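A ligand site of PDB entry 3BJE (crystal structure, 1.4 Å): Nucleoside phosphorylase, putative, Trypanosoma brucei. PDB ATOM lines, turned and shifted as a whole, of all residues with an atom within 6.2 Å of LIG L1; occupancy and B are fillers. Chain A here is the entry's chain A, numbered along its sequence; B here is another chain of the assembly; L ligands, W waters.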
ATOM      1  N   PHE A  48      20.746  28.849  15.454  1.00  0.00           N
ATOM      2  CA  PHE A  48      20.953  27.784  14.483  1.00  0.00           C
ATOM      3  C   PHE A  48      22.226  28.075  13.707  1.00  0.00           C
ATOM      4  O   PHE A  48      22.462  29.206  13.251  1.00  0.00           O
ATOM      5  CB  PHE A  48      19.831  27.712  13.458  1.00  0.00           C
ATOM      6  CG  PHE A  48      18.560  27.043  13.910  1.00  0.00           C
ATOM      7  CD1 PHE A  48      18.491  26.209  15.008  1.00  0.00           C
ATOM      8  CD2 PHE A  48      17.445  27.199  13.117  1.00  0.00           C
ATOM      9  CE1 PHE A  48      17.287  25.597  15.330  1.00  0.00           C
ATOM     10  CE2 PHE A  48      16.256  26.586  13.438  1.00  0.00           C
ATOM     11  CZ  PHE A  48      16.177  25.788  14.536  1.00  0.00           C
ATOM     12  N   VAL A  49      23.044  27.057  13.520  1.00  0.00           N
ATOM     13  CA  VAL A  49      24.175  27.122  12.597  1.00  0.00           C
ATOM     14  C   VAL A  49      24.091  25.932  11.683  1.00  0.00           C
ATOM     15  O   VAL A  49      23.583  24.908  12.058  1.00  0.00           O
ATOM     16  CB  VAL A  49      25.528  27.121  13.345  1.00  0.00           C
ATOM     17  CG1 VAL A  49      25.644  28.386  14.197  1.00  0.00           C
ATOM     18  CG2 VAL A  49      25.695  25.852  14.193  1.00  0.00           C
ATOM     19  N   GLY A  50      24.576  26.028  10.452  1.00  0.00           N
ATOM     20  CA  GLY A  50      24.522  24.866   9.588  1.00  0.00           C
ATOM     21  C   GLY A  50      25.631  23.874   9.908  1.00  0.00           C
ATOM     22  O   GLY A  50      25.405  22.646   9.954  1.00  0.00           O
ATOM     23  N   ASP A  51      26.823  24.398  10.080  1.00  0.00           N
ATOM     24  CA  ASP A  51      28.031  23.616  10.239  1.00  0.00           C
ATOM     25  C   ASP A  51      28.176  23.150  11.691  1.00  0.00           C
ATOM     26  O   ASP A  51      28.262  23.984  12.592  1.00  0.00           O
ATOM     27  CB  ASP A  51      29.214  24.496   9.860  1.00  0.00           C
ATOM     28  CG  ASP A  51      30.549  23.775   9.899  1.00  0.00           C
ATOM     29  OD1 ASP A  51      30.625  22.597  10.307  1.00  0.00           O
ATOM     30  OD2 ASP A  51      31.558  24.410   9.532  1.00  0.00           O
ATOM     31  N   ARG A  54      30.706  24.838  13.991  1.00  0.00           N
ATOM     32  CA  ARG A  54      30.499  26.187  14.538  1.00  0.00           C
ATOM     33  C   ARG A  54      29.904  26.174  15.953  1.00  0.00           C
ATOM     34  O   ARG A  54      29.890  27.212  16.633  1.00  0.00           O
ATOM     35  CB  ARG A  54      29.606  27.002  13.592  1.00  0.00           C
ATOM     36  CG  ARG A  54      29.659  28.529  13.821  1.00  0.00           C
ATOM     37  CD  ARG A  54      28.932  29.342  12.733  1.00  0.00           C
ATOM     38  NE  ARG A  54      29.351  28.942  11.392  1.00  0.00           N
ATOM     39  CZ  ARG A  54      28.540  28.668  10.372  1.00  0.00           C
ATOM     40  NH1 ARG A  54      27.222  28.762  10.468  1.00  0.00           N
ATOM     41  NH2 ARG A  54      29.068  28.272   9.222  1.00  0.00           N
ATOM     42  N   GLY A  94      22.845  21.104  10.221  1.00  0.00           N
ATOM     43  CA  GLY A  94      23.290  20.593   8.934  1.00  0.00           C
ATOM     44  C   GLY A  94      22.681  21.443   7.834  1.00  0.00           C
ATOM     45  O   GLY A  94      22.049  22.463   8.099  1.00  0.00           O
ATOM     46  N   MET A  95      22.830  20.993   6.592  1.00  0.00           N
ATOM     47  CA  MET A  95      22.489  21.832   5.453  1.00  0.00           C
ATOM     48  C   MET A  95      21.057  21.632   5.008  1.00  0.00           C
ATOM     49  O   MET A  95      20.618  20.495   4.862  1.00  0.00           O
ATOM     50  CB  MET A  95      23.440  21.546   4.308  1.00  0.00           C
ATOM     51  CG  MET A  95      24.866  21.750   4.688  1.00  0.00           C
ATOM     52  SD  MET A  95      26.023  21.594   3.321  1.00  0.00           S
ATOM     53  CE  MET A  95      26.056  19.825   3.130  1.00  0.00           C
ATOM     54  N   GLY A  96      20.337  22.729   4.803  1.00  0.00           N
ATOM     55  CA  GLY A  96      19.075  22.680   4.101  1.00  0.00           C
ATOM     56  C   GLY A  96      17.770  22.870   4.866  1.00  0.00           C
ATOM     57  O   GLY A  96      17.701  22.680   6.078  1.00  0.00           O
ATOM     58  N   ARG A 145      19.230  32.174  12.986  1.00  0.00           N
ATOM     59  CA  ARG A 145      20.263  31.500  12.202  1.00  0.00           C
ATOM     60  C   ARG A 145      21.448  32.421  12.031  1.00  0.00           C
ATOM     61  O   ARG A 145      21.278  33.572  11.661  1.00  0.00           O
ATOM     62  CB  ARG A 145      19.699  31.101  10.839  1.00  0.00           C
ATOM     63  CG  ARG A 145      20.775  30.751   9.819  1.00  0.00           C
ATOM     64  CD  ARG A 145      20.184  30.036   8.621  1.00  0.00           C
ATOM     65  NE  ARG A 145      21.073  30.118   7.453  1.00  0.00           N
ATOM     66  CZ  ARG A 145      22.273  29.544   7.369  1.00  0.00           C
ATOM     67  NH1 ARG A 145      22.987  29.714   6.269  1.00  0.00           N
ATOM     68  NH2 ARG A 145      22.780  28.808   8.365  1.00  0.00           N
ATOM     69  N   LEU A 146      22.639  31.913  12.329  1.00  0.00           N
ATOM     70  CA  LEU A 146      23.888  32.601  12.005  1.00  0.00           C
ATOM     71  C   LEU A 146      24.630  31.694  11.031  1.00  0.00           C
ATOM     72  O   LEU A 146      25.110  30.615  11.405  1.00  0.00           O
ATOM     73  CB  LEU A 146      24.742  32.888  13.247  1.00  0.00           C
ATOM     74  CG  LEU A 146      26.156  33.445  12.964  1.00  0.00           C
ATOM     75  CD1 LEU A 146      26.151  34.685  12.044  1.00  0.00           C
ATOM     76  CD2 LEU A 146      26.882  33.757  14.262  1.00  0.00           C
ATOM     77  N   GLY A 147      24.673  32.102   9.764  1.00  0.00           N
ATOM     78  CA  GLY A 147      25.158  31.243   8.714  1.00  0.00           C
ATOM     79  C   GLY A 147      26.169  31.877   7.794  1.00  0.00           C
ATOM     80  O   GLY A 147      26.753  32.919   8.109  1.00  0.00           O
ATOM     81  N   THR A 148      26.413  31.198   6.680  1.00  0.00           N
ATOM     82  CA  THR A 148      27.206  31.749   5.596  1.00  0.00           C
ATOM     83  C   THR A 148      26.317  31.786   4.371  1.00  0.00           C
ATOM     84  O   THR A 148      25.309  31.114   4.312  1.00  0.00           O
ATOM     85  CB  THR A 148      28.467  30.904   5.300  1.00  0.00           C
ATOM     86  OG1 THR A 148      28.103  29.569   4.911  1.00  0.00           O
ATOM     87  CG2 THR A 148      29.417  30.900   6.527  1.00  0.00           C
ATOM     88  N   CYS A 149      26.682  32.605   3.395  1.00  0.00           N
ATOM     89  CA  CYS A 149      25.822  32.728   2.215  1.00  0.00           C
ATOM     90  C   CYS A 149      26.550  33.289   1.022  1.00  0.00           C
ATOM     91  O   CYS A 149      27.708  33.716   1.110  1.00  0.00           O
ATOM     92  CB  CYS A 149      24.640  33.645   2.555  1.00  0.00           C
ATOM     93  SG  CYS A 149      25.169  35.381   2.844  1.00  0.00           S
ATOM     94  N   PHE A 250      23.066  23.645  -3.780  1.00  0.00           N
ATOM     95  CA  PHE A 250      24.156  24.608  -3.788  1.00  0.00           C
ATOM     96  C   PHE A 250      24.611  25.034  -5.195  1.00  0.00           C
ATOM     97  O   PHE A 250      25.130  26.126  -5.384  1.00  0.00           O
ATOM     98  CB  PHE A 250      25.342  23.998  -3.061  1.00  0.00           C
ATOM     99  CG  PHE A 250      26.479  24.950  -2.844  1.00  0.00           C
ATOM    100  CD1 PHE A 250      26.482  25.761  -1.721  1.00  0.00           C
ATOM    101  CD2 PHE A 250      27.544  25.025  -3.712  1.00  0.00           C
ATOM    102  CE1 PHE A 250      27.525  26.632  -1.477  1.00  0.00           C
ATOM    103  CE2 PHE A 250      28.599  25.878  -3.468  1.00  0.00           C
ATOM    104  CZ  PHE A 250      28.593  26.689  -2.357  1.00  0.00           C
ATOM    105  N   GLN A 254      21.432  26.978  -7.202  1.00  0.00           N
ATOM    106  CA  GLN A 254      21.789  28.383  -7.002  1.00  0.00           C
ATOM    107  C   GLN A 254      22.334  29.040  -8.295  1.00  0.00           C
ATOM    108  O   GLN A 254      22.965  30.063  -8.238  1.00  0.00           O
ATOM    109  CB  GLN A 254      22.764  28.554  -5.834  1.00  0.00           C
ATOM    110  CG  GLN A 254      22.224  28.025  -4.512  1.00  0.00           C
ATOM    111  CD  GLN A 254      23.096  28.304  -3.292  1.00  0.00           C
ATOM    112  OE1 GLN A 254      23.907  29.261  -3.295  1.00  0.00           O
ATOM    113  NE2 GLN A 254      22.906  27.507  -2.237  1.00  0.00           N
ATOM    114  N   ILE A 291      21.829  34.629  -0.858  1.00  0.00           N
ATOM    115  CA  ILE A 291      21.310  33.308  -1.243  1.00  0.00           C
ATOM    116  C   ILE A 291      21.963  32.271  -0.340  1.00  0.00           C
ATOM    117  O   ILE A 291      23.196  32.283  -0.172  1.00  0.00           O
ATOM    118  CB  ILE A 291      21.673  32.952  -2.707  1.00  0.00           C
ATOM    119  CG1 ILE A 291      21.138  33.995  -3.673  1.00  0.00           C
ATOM    120  CG2 ILE A 291      21.185  31.523  -3.067  1.00  0.00           C
ATOM    121  CD1 ILE A 291      21.791  33.954  -5.071  1.00  0.00           C
ATOM    122  N   GLU A 292      21.164  31.371   0.210  1.00  0.00           N
ATOM    123  CA  GLU A 292      21.666  30.299   1.078  1.00  0.00           C
ATOM    124  C   GLU A 292      20.637  29.143   1.092  1.00  0.00           C
ATOM    125  O   GLU A 292      19.793  29.045   0.174  1.00  0.00           O
ATOM    126  CB  GLU A 292      22.048  30.821   2.471  1.00  0.00           C
ATOM    127  CG  GLU A 292      21.009  31.737   3.152  1.00  0.00           C
ATOM    128  CD  GLU A 292      19.786  30.963   3.573  1.00  0.00           C
ATOM    129  OE1 GLU A 292      19.831  30.394   4.692  1.00  0.00           O
ATOM    130  OE2 GLU A 292      18.824  30.919   2.775  1.00  0.00           O
ATOM    131  N   MET A 293      20.697  28.266   2.098  1.00  0.00           N
ATOM    132  CA  MET A 293      19.934  27.010   2.025  1.00  0.00           C
ATOM    133  C   MET A 293      18.949  26.706   3.161  1.00  0.00           C
ATOM    134  O   MET A 293      18.352  25.629   3.164  1.00  0.00           O
ATOM    135  CB  MET A 293      20.913  25.832   1.864  1.00  0.00           C
ATOM    136  CG  MET A 293      21.695  25.889   0.571  1.00  0.00           C
ATOM    137  SD  MET A 293      22.883  24.560   0.333  1.00  0.00           S
ATOM    138  CE  MET A 293      21.774  23.109   0.267  1.00  0.00           C
ATOM    139  N   GLU A 294      18.750  27.630   4.111  1.00  0.00           N
ATOM    140  CA  GLU A 294      17.888  27.364   5.284  1.00  0.00           C
ATOM    141  C   GLU A 294      16.813  28.385   5.642  1.00  0.00           C
ATOM    142  O   GLU A 294      15.822  28.042   6.279  1.00  0.00           O
ATOM    143  CB  GLU A 294      18.777  27.152   6.525  1.00  0.00           C
ATOM    144  CG  GLU A 294      19.622  25.867   6.468  1.00  0.00           C
ATOM    145  CD  GLU A 294      21.041  26.078   5.939  1.00  0.00           C
ATOM    146  OE1 GLU A 294      21.627  27.151   6.142  1.00  0.00           O
ATOM    147  OE2 GLU A 294      21.609  25.146   5.293  1.00  0.00           O
ATOM    148  N   CYS A 313      23.637  36.112   7.844  1.00  0.00           N
ATOM    149  CA  CYS A 313      24.648  35.232   7.281  1.00  0.00           C
ATOM    150  C   CYS A 313      25.833  36.013   6.747  1.00  0.00           C
ATOM    151  O   CYS A 313      25.642  37.018   6.099  1.00  0.00           O
ATOM    152  CB  CYS A 313      24.056  34.419   6.129  1.00  0.00           C
ATOM    153  SG  CYS A 313      22.661  33.358   6.568  1.00  0.00           S
ATOM    154  N   LEU B  33      34.447  21.540  -2.186  1.00  0.00           N
ATOM    155  CA  LEU B  33      34.105  22.417  -1.088  1.00  0.00           C
ATOM    156  C   LEU B  33      33.535  21.721   0.151  1.00  0.00           C
ATOM    157  O   LEU B  33      33.810  22.142   1.286  1.00  0.00           O
ATOM    158  CB  LEU B  33      33.124  23.468  -1.588  1.00  0.00           C
ATOM    159  CG  LEU B  33      32.751  24.639  -0.702  1.00  0.00           C
ATOM    160  CD1 LEU B  33      34.000  25.416  -0.261  1.00  0.00           C
ATOM    161  CD2 LEU B  33      31.796  25.551  -1.444  1.00  0.00           C
ATOM    162  N   HIS B  34      32.719  20.699  -0.061  1.00  0.00           N
ATOM    163  CA  HIS B  34      32.041  19.988   1.019  1.00  0.00           C
ATOM    164  C   HIS B  34      32.621  18.587   1.210  1.00  0.00           C
ATOM    165  O   HIS B  34      33.032  18.210   2.309  1.00  0.00           O
ATOM    166  CB  HIS B  34      30.521  19.921   0.755  1.00  0.00           C
ATOM    167  CG  HIS B  34      29.897  21.282   0.602  1.00  0.00           C
ATOM    168  ND1 HIS B  34      29.912  21.980  -0.587  1.00  0.00           N
ATOM    169  CD2 HIS B  34      29.269  22.078   1.498  1.00  0.00           C
ATOM    170  CE1 HIS B  34      29.312  23.145  -0.423  1.00  0.00           C
ATOM    171  NE2 HIS B  34      28.909  23.226   0.837  1.00  0.00           N
ATOM    172  N   ARG B  74      31.971  18.868   7.970  1.00  0.00           N
ATOM    173  CA  ARG B  74      30.515  18.994   8.155  1.00  0.00           C
ATOM    174  C   ARG B  74      29.919  17.555   8.301  1.00  0.00           C
ATOM    175  O   ARG B  74      30.514  16.702   8.926  1.00  0.00           O
ATOM    176  CB  ARG B  74      29.874  19.753   6.979  1.00  0.00           C
ATOM    177  CG  ARG B  74      30.229  21.225   6.891  1.00  0.00           C
ATOM    178  CD  ARG B  74      29.690  21.815   5.582  1.00  0.00           C
ATOM    179  NE  ARG B  74      29.877  23.272   5.472  1.00  0.00           N
ATOM    180  CZ  ARG B  74      29.035  24.187   5.955  1.00  0.00           C
ATOM    181  NH1 ARG B  74      27.955  23.809   6.609  1.00  0.00           N
ATOM    182  NH2 ARG B  74      29.288  25.488   5.773  1.00  0.00           N
ATOM    183  N   ILE B 102      24.677  18.576  -3.710  1.00  0.00           N
ATOM    184  CA  ILE B 102      26.053  18.994  -3.403  1.00  0.00           C
ATOM    185  C   ILE B 102      27.062  17.883  -3.720  1.00  0.00           C
ATOM    186  O   ILE B 102      28.046  18.114  -4.437  1.00  0.00           O
ATOM    187  CB  ILE B 102      26.167  19.430  -1.922  1.00  0.00           C
ATOM    188  CG1 ILE B 102      25.443  20.780  -1.722  1.00  0.00           C
ATOM    189  CG2 ILE B 102      27.637  19.497  -1.486  1.00  0.00           C
ATOM    190  CD1 ILE B 102      25.199  21.168  -0.253  1.00  0.00           C
HETATM  191  C1  LIG L   1      26.426  25.360   2.187  1.00  0.00           C
HETATM  192  O1  LIG L   1      27.853  25.466   2.061  1.00  0.00           O
HETATM  193  C2  LIG L   1      25.981  25.678   3.594  1.00  0.00           C
HETATM  194  O2  LIG L   1      26.533  26.922   4.054  1.00  0.00           O
HETATM  195  C3  LIG L   1      25.495  27.839   4.407  1.00  0.00           C
HETATM  196  C4  LIG L   1      24.293  27.336   3.603  1.00  0.00           C
HETATM  197  O3  LIG L   1      22.988  27.823   3.997  1.00  0.00           O
HETATM  198  C5  LIG L   1      24.477  25.820   3.701  1.00  0.00           C
HETATM  199  O4  LIG L   1      24.048  25.298   4.972  1.00  0.00           O
HETATM  200  O5  LIG L   1      25.269  27.944   5.856  1.00  0.00           O
HETATM  201  P1  LIG L   1      26.122  27.311   7.064  1.00  0.00           P
HETATM  202  O6  LIG L   1      25.892  25.818   6.805  1.00  0.00           O
HETATM  203  O7  LIG L   1      25.440  27.834   8.311  1.00  0.00           O
HETATM  204  O8  LIG L   1      27.569  27.688   6.922  1.00  0.00           O
HETATM  205  N1  LG2 L   2      26.261  29.160   1.132  1.00  0.00           N
HETATM  206  C1  LG2 L   2      25.374  29.012   0.121  1.00  0.00           C
HETATM  207  O1  LG2 L   2      24.316  28.313   0.267  1.00  0.00           O
HETATM  208  N2  LG2 L   2      25.609  29.573  -1.056  1.00  0.00           N
HETATM  209  C2  LG2 L   2      26.729  30.298  -1.271  1.00  0.00           C
HETATM  210  O2  LG2 L   2      26.883  30.806  -2.394  1.00  0.00           O
HETATM  211  C3  LG2 L   2      27.653  30.452  -0.258  1.00  0.00           C
HETATM  212  C4  LG2 L   2      27.396  29.861   0.958  1.00  0.00           C
HETATM  213  O   HOH W   1      29.296  27.627   2.848  1.00  0.00           O
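The side-chain carboxylate (OE2) of Glu 294 lies within hydrogen-bond range of an oxygen (O4) of LIG L1 (2.5 Å).
A ring nitrogen (NE2) of His 34 of chain B sits at hydrogen-bond distance from an oxygen (O1) of LIG L1, 2.8 Å away.
The side-chain hydroxyl (OG1) of Thr 148 sits at hydrogen-bond distance from an oxygen (O8) of LIG L1 (2.8 Å).
An oxygen (O8) of LIG L1 is in salt-bridge range of the guanidinium group (NH2) of Arg 54 (2.8 Å).
The guanidinium group (NH2) of Arg 145 lies within salt-bridge range of an oxygen (O7) of LIG L1.
An oxygen (O6) of LIG L1 is in salt-bridge range of the guanidinium group of Arg 74 of chain B (2.9 Å).
The backbone NH (N) of Gly 50 is in hydrogen-bond range of an oxygen (O7) of LIG L1 (2.9 Å).
The backbone NH (N) of Met 293 lies within hydrogen-bond range of an oxygen (O3) of LIG L1.
The side-chain amide oxygen of Gln 254 lies within hydrogen-bond range of a nitrogen (N2) of LG2 L2 (2.8 Å).
The guanidinium group (NH1) of Arg 145 is in salt-bridge range of the side-chain carboxylate (OE1) of Glu 294 (2.9 Å).
The backbone NH (N) of Glu 294 is in hydrogen-bond range of the side-chain carboxylate (OE1) of Glu 292 (3.0 Å).
The side-chain carboxylate (OE2) of Glu 294 sits at hydrogen-bond distance from the backbone NH (N) of Gly 96.
NH1 of Arg 145 lies within hydrogen-bond range of O of Thr 148 (3.3 Å).
The guanidinium group of Arg 54 is in hydrogen-bond range of the backbone carbonyl oxygen of Leu 146.
NE of Arg 145 is in salt-bridge range of OE1 of Glu 292, at 3.0 Å.
NH1 of Arg 145 is in hydrogen-bond range of SG of Cys 313, 3.7 Å away.
The backbone NH (N) of Gly 94 sits at hydrogen-bond distance from the backbone carbonyl oxygen (O) of Gly 50, 3.0 Å away.
Asp 51 touches LIG L1.
Met 95 touches LIG L1 (CG to O4, 3.7 Å).
Gly 147 touches LIG L1 (CA to O7, 3.4 Å).
CE1 of Phe 250 touches O1 of LIG L1 (3.7 Å).
Glu 292 touches LIG L1 (CB to O3, 3.5 Å).
Hydrophobic or aromatic side chains that line LIG L1: Met 95, Phe 250, Met 293 and His 34 of chain B.
13 residues have an atom within 4 Å of LIG L1: Gly 50, Asp 51, Arg 54, Met 95, Arg 145, Gly 147, Thr 148, Phe 250, Glu 292, Met 293, Glu 294, His 34 of chain B and Arg 74 of chain B.
The nearest printed residue that does not touch LIG L1 is Val 49 (4.1 Å).
Water W1 lies within hydrogen-bond range of an oxygen (O1) of LIG L1 (2.7 Å) and the side-chain hydroxyl of Thr 148 (3.1 Å).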
